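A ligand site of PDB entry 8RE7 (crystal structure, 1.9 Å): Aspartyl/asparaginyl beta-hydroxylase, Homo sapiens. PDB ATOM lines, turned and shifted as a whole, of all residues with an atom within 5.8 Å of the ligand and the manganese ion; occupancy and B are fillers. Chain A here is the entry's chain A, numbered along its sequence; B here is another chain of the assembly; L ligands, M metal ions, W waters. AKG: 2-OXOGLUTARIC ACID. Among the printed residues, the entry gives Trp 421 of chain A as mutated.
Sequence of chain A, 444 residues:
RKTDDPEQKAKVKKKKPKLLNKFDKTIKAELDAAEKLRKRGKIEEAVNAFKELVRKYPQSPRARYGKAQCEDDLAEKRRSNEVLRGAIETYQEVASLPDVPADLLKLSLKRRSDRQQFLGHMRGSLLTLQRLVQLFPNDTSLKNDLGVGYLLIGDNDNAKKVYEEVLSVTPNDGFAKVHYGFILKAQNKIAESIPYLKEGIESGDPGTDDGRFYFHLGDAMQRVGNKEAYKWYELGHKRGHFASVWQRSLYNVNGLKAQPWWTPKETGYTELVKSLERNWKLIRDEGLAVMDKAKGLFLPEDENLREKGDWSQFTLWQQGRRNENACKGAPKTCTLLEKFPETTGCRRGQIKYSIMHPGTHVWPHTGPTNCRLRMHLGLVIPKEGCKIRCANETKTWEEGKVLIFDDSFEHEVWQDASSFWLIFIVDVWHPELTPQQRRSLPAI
An oxygen (O2) of the ligand lies within salt-bridge range of the guanidinium group (NH1) of Arg 374, 3.9 Å away. NE1 of Trp 311 is in hydrogen-bond range of O4 of the ligand. A ring nitrogen (NE2) of His 376 sits at hydrogen-bond distance from an oxygen (O2) of the ligand (2.6 Å). The side-chain amide nitrogen (NE2) of Gln 313 is in hydrogen-bond range of an oxygen (O4) of the ligand, at 2.8 Å. O4 of the ligand sits at hydrogen-bond distance from OG of Ser 354.
The guanidinium group (NH1) of Arg 374 lies within salt-bridge range of the side-chain carboxylate (OD1) of Asp 18 of chain B. The guanidinium group of Arg 374 is in salt-bridge range of the side-chain carboxylate of Asp 407 (3.5 Å). NE2 of Gln 313 sits close to NZ of Lys 352, 3.5 Å away. OD2 of Asp 18 of chain B sits at hydrogen-bond distance from NE2 of Gln 313, at 2.9 Å. The backbone NH of Arg 374 is in hydrogen-bond range of the backbone carbonyl oxygen of Phe 405 (2.9 Å). O of Val 413 lies within hydrogen-bond range of N of Val 362 (2.9 Å). The backbone carbonyl oxygen (O) of Trp 311 lies within hydrogen-bond range of the backbone NH (N) of Glu 301, at 3.0 Å. The backbone NH (N) of Ser 354 is in hydrogen-bond range of the backbone carbonyl oxygen (O) of Ile 423, at 3.0 Å.
Residues that only touch the ligand: Met 356 (3.9 Å), Phe 405 (3.7 Å), Val 413 (3.99 Å), Ile 425 (3.4 Å) and Asp 18 of chain B (3.9 Å). Hydrophobic or aromatic side chains within 4 Å of the ligand: Trp 311, Met 356, His 365, His 376, Phe 405, His 411, Val 413 and Ile 425. 12 residues have an atom within 4 Å of the ligand: Trp 311, Gln 313, Ser 354, Met 356, His 365, Arg 374, His 376, Phe 405, His 411, Val 413, Ile 425 and Asp 18 of chain B.
The nearest printed residue that does not touch the manganese ion is Arg 374 (4.1 Å).
The manganese ion is bound by water W1, a ring nitrogen (NE2) of His 411, an oxygen (O1) of the ligand, water W2, a ring nitrogen (NE2) of His 365 and an oxygen (O5) of the ligand.
Water W1 lies within hydrogen-bond range of OD2 of Asp 407, O of Asp 18 of chain B and NH1 of Arg 374. Water W2 bridges an oxygen (O3) of the ligand (2.7 Å) and the side-chain carboxylate of Asp 18 of chain B (3.4 Å).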
ATOM      1  N   GLU A 301       9.221 -12.104 -12.818  1.00  0.00           N
ATOM      2  CA  GLU A 301       8.306 -13.220 -13.007  1.00  0.00           C
ATOM      3  C   GLU A 301       7.119 -12.718 -13.817  1.00  0.00           C
ATOM      4  O   GLU A 301       6.529 -11.687 -13.476  1.00  0.00           O
ATOM      5  CB  GLU A 301       7.831 -13.767 -11.655  1.00  0.00           C
ATOM      6  CG  GLU A 301       7.469 -15.259 -11.639  1.00  0.00           C
ATOM      7  CD  GLU A 301       6.033 -15.522 -12.097  1.00  0.00           C
ATOM      8  OE1 GLU A 301       5.269 -14.565 -12.354  1.00  0.00           O
ATOM      9  OE2 GLU A 301       5.664 -16.714 -12.180  1.00  0.00           O
ATOM     10  N   LEU A 305       1.438 -13.512 -11.516  1.00  0.00           N
ATOM     11  CA  LEU A 305       1.277 -14.024 -10.171  1.00  0.00           C
ATOM     12  C   LEU A 305       1.681 -13.026  -9.090  1.00  0.00           C
ATOM     13  O   LEU A 305       1.463 -13.288  -7.902  1.00  0.00           O
ATOM     14  CB  LEU A 305       2.097 -15.309 -10.000  1.00  0.00           C
ATOM     15  CG  LEU A 305       1.694 -16.421 -10.953  1.00  0.00           C
ATOM     16  CD1 LEU A 305       2.600 -17.612 -10.756  1.00  0.00           C
ATOM     17  CD2 LEU A 305       0.240 -16.822 -10.709  1.00  0.00           C
ATOM     18  N   TRP A 311       9.809  -8.921  -8.035  1.00  0.00           N
ATOM     19  CA  TRP A 311      10.032 -10.362  -7.894  1.00  0.00           C
ATOM     20  C   TRP A 311      10.619 -10.867  -9.197  1.00  0.00           C
ATOM     21  O   TRP A 311       9.968 -10.787 -10.236  1.00  0.00           O
ATOM     22  CB  TRP A 311       8.701 -11.071  -7.571  1.00  0.00           C
ATOM     23  CG  TRP A 311       8.663 -12.590  -7.678  1.00  0.00           C
ATOM     24  CD1 TRP A 311       9.684 -13.462  -7.475  1.00  0.00           C
ATOM     25  CD2 TRP A 311       7.503 -13.378  -7.990  1.00  0.00           C
ATOM     26  NE1 TRP A 311       9.233 -14.764  -7.654  1.00  0.00           N
ATOM     27  CE2 TRP A 311       7.894 -14.724  -7.962  1.00  0.00           C
ATOM     28  CE3 TRP A 311       6.169 -13.068  -8.282  1.00  0.00           C
ATOM     29  CZ2 TRP A 311       7.002 -15.766  -8.215  1.00  0.00           C
ATOM     30  CZ3 TRP A 311       5.289 -14.083  -8.539  1.00  0.00           C
ATOM     31  CH2 TRP A 311       5.709 -15.427  -8.515  1.00  0.00           C
ATOM     32  N   SER A 312      11.840 -11.390  -9.157  1.00  0.00           N
ATOM     33  CA  SER A 312      12.527 -11.811 -10.366  1.00  0.00           C
ATOM     34  C   SER A 312      13.250 -13.111 -10.080  1.00  0.00           C
ATOM     35  O   SER A 312      13.477 -13.466  -8.926  1.00  0.00           O
ATOM     36  CB  SER A 312      13.488 -10.711 -10.867  1.00  0.00           C
ATOM     37  OG  SER A 312      14.473 -10.429  -9.879  1.00  0.00           O
ATOM     38  N   GLN A 313      13.585 -13.833 -11.151  1.00  0.00           N
ATOM     39  CA  GLN A 313      14.139 -15.176 -11.062  1.00  0.00           C
ATOM     40  C   GLN A 313      15.265 -15.334 -12.076  1.00  0.00           C
ATOM     41  O   GLN A 313      15.203 -14.796 -13.185  1.00  0.00           O
ATOM     42  CB  GLN A 313      13.073 -16.254 -11.349  1.00  0.00           C
ATOM     43  CG  GLN A 313      11.960 -16.342 -10.338  1.00  0.00           C
ATOM     44  CD  GLN A 313      10.721 -16.968 -10.970  1.00  0.00           C
ATOM     45  OE1 GLN A 313      10.482 -16.792 -12.176  1.00  0.00           O
ATOM     46  NE2 GLN A 313       9.915 -17.674 -10.168  1.00  0.00           N
ATOM     47  N   LYS A 352      16.174 -22.527 -10.199  1.00  0.00           N
ATOM     48  CA  LYS A 352      16.304 -21.085 -10.371  1.00  0.00           C
ATOM     49  C   LYS A 352      16.515 -20.395  -9.036  1.00  0.00           C
ATOM     50  O   LYS A 352      15.964 -20.816  -8.015  1.00  0.00           O
ATOM     51  CB  LYS A 352      15.047 -20.493 -11.067  1.00  0.00           C
ATOM     52  CG  LYS A 352      13.731 -20.714 -10.316  1.00  0.00           C
ATOM     53  CD  LYS A 352      12.526 -20.636 -11.313  1.00  0.00           C
ATOM     54  CE  LYS A 352      11.188 -20.862 -10.625  1.00  0.00           C
ATOM     55  NZ  LYS A 352      10.033 -20.858 -11.605  1.00  0.00           N
ATOM     56  N   TYR A 353      17.329 -19.335  -9.048  1.00  0.00           N
ATOM     57  CA  TYR A 353      17.293 -18.383  -7.948  1.00  0.00           C
ATOM     58  C   TYR A 353      16.023 -17.548  -8.018  1.00  0.00           C
ATOM     59  O   TYR A 353      15.500 -17.268  -9.094  1.00  0.00           O
ATOM     60  CB  TYR A 353      18.494 -17.437  -8.010  1.00  0.00           C
ATOM     61  CG  TYR A 353      19.867 -18.070  -7.803  1.00  0.00           C
ATOM     62  CD1 TYR A 353      20.462 -18.111  -6.559  1.00  0.00           C
ATOM     63  CD2 TYR A 353      20.590 -18.553  -8.883  1.00  0.00           C
ATOM     64  CE1 TYR A 353      21.739 -18.660  -6.375  1.00  0.00           C
ATOM     65  CE2 TYR A 353      21.829 -19.081  -8.723  1.00  0.00           C
ATOM     66  CZ  TYR A 353      22.418 -19.122  -7.472  1.00  0.00           C
ATOM     67  OH  TYR A 353      23.668 -19.650  -7.329  1.00  0.00           O
ATOM     68  N   SER A 354      15.576 -17.070  -6.851  1.00  0.00           N
ATOM     69  CA  SER A 354      14.428 -16.182  -6.766  1.00  0.00           C
ATOM     70  C   SER A 354      14.740 -15.052  -5.800  1.00  0.00           C
ATOM     71  O   SER A 354      15.233 -15.307  -4.705  1.00  0.00           O
ATOM     72  CB  SER A 354      13.198 -16.937  -6.247  1.00  0.00           C
ATOM     73  OG  SER A 354      12.035 -16.138  -6.295  1.00  0.00           O
ATOM     74  N   MET A 356      13.038 -11.364  -4.043  1.00  0.00           N
ATOM     75  CA  MET A 356      11.932 -10.457  -3.798  1.00  0.00           C
ATOM     76  C   MET A 356      12.410  -9.341  -2.878  1.00  0.00           C
ATOM     77  O   MET A 356      13.245  -9.571  -2.000  1.00  0.00           O
ATOM     78  CB  MET A 356      10.745 -11.158  -3.151  1.00  0.00           C
ATOM     79  CG  MET A 356      10.094 -12.239  -4.016  1.00  0.00           C
ATOM     80  SD  MET A 356       8.772 -13.018  -3.079  1.00  0.00           S
ATOM     81  CE  MET A 356       8.488 -14.513  -4.055  1.00  0.00           C
ATOM     82  N   VAL A 362       2.923 -12.196  -3.490  1.00  0.00           N
ATOM     83  CA  VAL A 362       2.542 -13.122  -4.553  1.00  0.00           C
ATOM     84  C   VAL A 362       1.110 -13.558  -4.308  1.00  0.00           C
ATOM     85  O   VAL A 362       0.791 -14.071  -3.235  1.00  0.00           O
ATOM     86  CB  VAL A 362       3.483 -14.335  -4.586  1.00  0.00           C
ATOM     87  CG1 VAL A 362       3.045 -15.326  -5.665  1.00  0.00           C
ATOM     88  CG2 VAL A 362       4.947 -13.915  -4.822  1.00  0.00           C
ATOM     89  N   HIS A 365      -1.815 -18.960  -5.484  1.00  0.00           N
ATOM     90  CA  HIS A 365      -1.806 -19.626  -6.781  1.00  0.00           C
ATOM     91  C   HIS A 365      -1.350 -21.064  -6.618  1.00  0.00           C
ATOM     92  O   HIS A 365      -0.880 -21.477  -5.558  1.00  0.00           O
ATOM     93  CB  HIS A 365      -0.876 -18.925  -7.777  1.00  0.00           C
ATOM     94  CG  HIS A 365       0.572 -19.050  -7.425  1.00  0.00           C
ATOM     95  ND1 HIS A 365       1.142 -18.347  -6.380  1.00  0.00           N
ATOM     96  CD2 HIS A 365       1.566 -19.794  -7.966  1.00  0.00           C
ATOM     97  CE1 HIS A 365       2.430 -18.648  -6.310  1.00  0.00           C
ATOM     98  NE2 HIS A 365       2.710 -19.522  -7.256  1.00  0.00           N
ATOM     99  N   GLY A 367       0.679 -24.330  -8.953  1.00  0.00           N
ATOM    100  CA  GLY A 367       1.444 -24.733 -10.110  1.00  0.00           C
ATOM    101  C   GLY A 367       0.658 -25.655 -11.033  1.00  0.00           C
ATOM    102  O   GLY A 367      -0.425 -26.141 -10.703  1.00  0.00           O
ATOM    103  N   ARG A 374       8.607 -28.937  -4.821  1.00  0.00           N
ATOM    104  CA  ARG A 374       9.444 -27.745  -4.933  1.00  0.00           C
ATOM    105  C   ARG A 374      10.258 -27.569  -3.654  1.00  0.00           C
ATOM    106  O   ARG A 374       9.683 -27.392  -2.574  1.00  0.00           O
ATOM    107  CB  ARG A 374       8.569 -26.525  -5.203  1.00  0.00           C
ATOM    108  CG  ARG A 374       9.330 -25.247  -5.409  1.00  0.00           C
ATOM    109  CD  ARG A 374       8.560 -24.341  -6.308  1.00  0.00           C
ATOM    110  NE  ARG A 374       8.822 -24.620  -7.720  1.00  0.00           N
ATOM    111  CZ  ARG A 374       8.417 -23.837  -8.708  1.00  0.00           C
ATOM    112  NH1 ARG A 374       7.711 -22.740  -8.464  1.00  0.00           N
ATOM    113  NH2 ARG A 374       8.775 -24.127  -9.948  1.00  0.00           N
ATOM    114  N   HIS A 376      13.014 -25.264  -1.521  1.00  0.00           N
ATOM    115  CA  HIS A 376      13.518 -23.909  -1.329  1.00  0.00           C
ATOM    116  C   HIS A 376      14.734 -23.977  -0.396  1.00  0.00           C
ATOM    117  O   HIS A 376      14.597 -24.432   0.740  1.00  0.00           O
ATOM    118  CB  HIS A 376      12.470 -23.004  -0.684  1.00  0.00           C
ATOM    119  CG  HIS A 376      11.436 -22.492  -1.645  1.00  0.00           C
ATOM    120  ND1 HIS A 376      10.485 -21.557  -1.271  1.00  0.00           N
ATOM    121  CD2 HIS A 376      11.185 -22.768  -2.940  1.00  0.00           C
ATOM    122  CE1 HIS A 376       9.710 -21.281  -2.299  1.00  0.00           C
ATOM    123  NE2 HIS A 376      10.121 -21.991  -3.332  1.00  0.00           N
ATOM    124  N   ILE A 388       5.820 -17.842   3.841  1.00  0.00           N
ATOM    125  CA  ILE A 388       5.153 -18.577   2.767  1.00  0.00           C
ATOM    126  C   ILE A 388       4.029 -19.418   3.376  1.00  0.00           C
ATOM    127  O   ILE A 388       4.239 -20.166   4.332  1.00  0.00           O
ATOM    128  CB  ILE A 388       6.126 -19.489   1.977  1.00  0.00           C
ATOM    129  CG1 ILE A 388       5.379 -20.377   0.985  1.00  0.00           C
ATOM    130  CG2 ILE A 388       6.917 -20.385   2.878  1.00  0.00           C
ATOM    131  CD1 ILE A 388       6.289 -21.020  -0.050  1.00  0.00           C
ATOM    132  N   PHE A 405       7.735 -28.112  -0.309  1.00  0.00           N
ATOM    133  CA  PHE A 405       6.282 -28.111  -0.394  1.00  0.00           C
ATOM    134  C   PHE A 405       5.880 -28.573  -1.773  1.00  0.00           C
ATOM    135  O   PHE A 405       6.688 -28.609  -2.704  1.00  0.00           O
ATOM    136  CB  PHE A 405       5.683 -26.726  -0.079  1.00  0.00           C
ATOM    137  CG  PHE A 405       6.106 -25.641  -1.032  1.00  0.00           C
ATOM    138  CD1 PHE A 405       7.358 -25.052  -0.945  1.00  0.00           C
ATOM    139  CD2 PHE A 405       5.233 -25.196  -2.021  1.00  0.00           C
ATOM    140  CE1 PHE A 405       7.747 -24.041  -1.817  1.00  0.00           C
ATOM    141  CE2 PHE A 405       5.614 -24.189  -2.899  1.00  0.00           C
ATOM    142  CZ  PHE A 405       6.871 -23.610  -2.808  1.00  0.00           C
ATOM    143  N   ASP A 407       3.923 -27.513  -4.771  1.00  0.00           N
ATOM    144  CA  ASP A 407       3.353 -26.247  -5.245  1.00  0.00           C
ATOM    145  C   ASP A 407       2.123 -26.458  -6.129  1.00  0.00           C
ATOM    146  O   ASP A 407       1.596 -25.477  -6.672  1.00  0.00           O
ATOM    147  CB  ASP A 407       4.426 -25.399  -5.948  1.00  0.00           C
ATOM    148  CG  ASP A 407       4.611 -25.744  -7.425  1.00  0.00           C
ATOM    149  OD1 ASP A 407       4.528 -26.927  -7.811  1.00  0.00           O
ATOM    150  OD2 ASP A 407       4.894 -24.807  -8.215  1.00  0.00           O
ATOM    151  N   HIS A 411      -0.635 -21.746  -2.768  1.00  0.00           N
ATOM    152  CA  HIS A 411       0.386 -21.174  -1.910  1.00  0.00           C
ATOM    153  C   HIS A 411       0.536 -19.689  -2.211  1.00  0.00           C
ATOM    154  O   HIS A 411       0.069 -19.187  -3.241  1.00  0.00           O
ATOM    155  CB  HIS A 411       1.721 -21.922  -2.058  1.00  0.00           C
ATOM    156  CG  HIS A 411       2.257 -21.941  -3.456  1.00  0.00           C
ATOM    157  ND1 HIS A 411       1.804 -22.818  -4.420  1.00  0.00           N
ATOM    158  CD2 HIS A 411       3.200 -21.181  -4.045  1.00  0.00           C
ATOM    159  CE1 HIS A 411       2.432 -22.584  -5.553  1.00  0.00           C
ATOM    160  NE2 HIS A 411       3.302 -21.600  -5.353  1.00  0.00           N
ATOM    161  N   VAL A 413       3.066 -15.967  -0.894  1.00  0.00           N
ATOM    162  CA  VAL A 413       4.315 -15.473  -0.308  1.00  0.00           C
ATOM    163  C   VAL A 413       4.197 -13.978  -0.054  1.00  0.00           C
ATOM    164  O   VAL A 413       3.637 -13.245  -0.870  1.00  0.00           O
ATOM    165  CB  VAL A 413       5.519 -15.794  -1.219  1.00  0.00           C
ATOM    166  CG1 VAL A 413       6.809 -15.186  -0.662  1.00  0.00           C
ATOM    167  CG2 VAL A 413       5.676 -17.307  -1.353  1.00  0.00           C
ATOM    168  N   TRP A 421      15.364 -10.497  -0.185  1.00  0.00           N
ATOM    169  CA  TRP A 421      15.193 -11.916   0.104  1.00  0.00           C
ATOM    170  C   TRP A 421      15.664 -12.683  -1.120  1.00  0.00           C
ATOM    171  O   TRP A 421      15.348 -12.306  -2.247  1.00  0.00           O
ATOM    172  CB  TRP A 421      13.707 -12.172   0.393  1.00  0.00           C
ATOM    173  CG  TRP A 421      13.130 -13.568   0.427  1.00  0.00           C
ATOM    174  CD1 TRP A 421      12.866 -14.307   1.538  1.00  0.00           C
ATOM    175  CD2 TRP A 421      12.587 -14.323  -0.687  1.00  0.00           C
ATOM    176  NE1 TRP A 421      12.232 -15.478   1.197  1.00  0.00           N
ATOM    177  CE2 TRP A 421      12.041 -15.513  -0.155  1.00  0.00           C
ATOM    178  CE3 TRP A 421      12.508 -14.096  -2.072  1.00  0.00           C
ATOM    179  CZ2 TRP A 421      11.450 -16.493  -0.963  1.00  0.00           C
ATOM    180  CZ3 TRP A 421      11.926 -15.094  -2.876  1.00  0.00           C
ATOM    181  CH2 TRP A 421      11.399 -16.257  -2.318  1.00  0.00           C
ATOM    182  N   ILE A 423      16.392 -16.840  -2.462  1.00  0.00           N
ATOM    183  CA  ILE A 423      16.355 -18.278  -2.228  1.00  0.00           C
ATOM    184  C   ILE A 423      16.794 -18.983  -3.506  1.00  0.00           C
ATOM    185  O   ILE A 423      16.920 -18.378  -4.571  1.00  0.00           O
ATOM    186  CB  ILE A 423      14.971 -18.794  -1.776  1.00  0.00           C
ATOM    187  CG1 ILE A 423      13.916 -18.617  -2.885  1.00  0.00           C
ATOM    188  CG2 ILE A 423      14.515 -18.116  -0.486  1.00  0.00           C
ATOM    189  CD1 ILE A 423      12.678 -19.473  -2.676  1.00  0.00           C
ATOM    190  N   ILE A 425      15.639 -22.292  -5.767  1.00  0.00           N
ATOM    191  CA  ILE A 425      14.484 -23.165  -5.983  1.00  0.00           C
ATOM    192  C   ILE A 425      14.958 -24.372  -6.769  1.00  0.00           C
ATOM    193  O   ILE A 425      15.585 -24.197  -7.822  1.00  0.00           O
ATOM    194  CB  ILE A 425      13.349 -22.437  -6.725  1.00  0.00           C
ATOM    195  CG1 ILE A 425      12.887 -21.225  -5.942  1.00  0.00           C
ATOM    196  CG2 ILE A 425      12.188 -23.373  -6.912  1.00  0.00           C
ATOM    197  CD1 ILE A 425      11.792 -20.450  -6.667  1.00  0.00           C
ATOM    198  N   ASP B  18       5.645 -21.446 -13.191  1.00  0.00           N
ATOM    199  CA  ASP B  18       5.087 -21.316 -11.850  1.00  0.00           C
ATOM    200  C   ASP B  18       3.580 -21.530 -11.789  1.00  0.00           C
ATOM    201  O   ASP B  18       3.058 -21.829 -10.708  1.00  0.00           O
ATOM    202  CB  ASP B  18       5.402 -19.922 -11.301  1.00  0.00           C
ATOM    203  CG  ASP B  18       6.887 -19.716 -11.101  1.00  0.00           C
ATOM    204  OD1 ASP B  18       7.546 -20.703 -10.723  1.00  0.00           O
ATOM    205  OD2 ASP B  18       7.387 -18.599 -11.355  1.00  0.00           O
HETATM  206  C1  AKG L   1       7.195 -20.717  -5.556  1.00  0.00           C
HETATM  207  O1  AKG L   1       6.483 -21.518  -6.161  1.00  0.00           O
HETATM  208  O2  AKG L   1       8.372 -21.020  -5.044  1.00  0.00           O
HETATM  209  C2  AKG L   1       6.695 -19.305  -5.270  1.00  0.00           C
HETATM  210  O5  AKG L   1       5.514 -19.073  -5.489  1.00  0.00           O
HETATM  211  C3  AKG L   1       7.617 -18.224  -4.718  1.00  0.00           C
HETATM  212  C4  AKG L   1       9.023 -18.210  -5.300  1.00  0.00           C
HETATM  213  C5  AKG L   1       9.128 -18.062  -6.795  1.00  0.00           C
HETATM  214  O3  AKG L   1       8.157 -18.621  -7.439  1.00  0.00           O
HETATM  215  O4  AKG L   1      10.081 -17.540  -7.352  1.00  0.00           O
HETATM  216 MN    MN M   1       4.604 -20.696  -6.801  1.00  0.00          MN
HETATM  217  O   HOH W   1       4.436 -22.210  -8.266  1.00  0.00           O
HETATM  218  O   HOH W   2       5.706 -19.395  -8.161  1.00  0.00           O
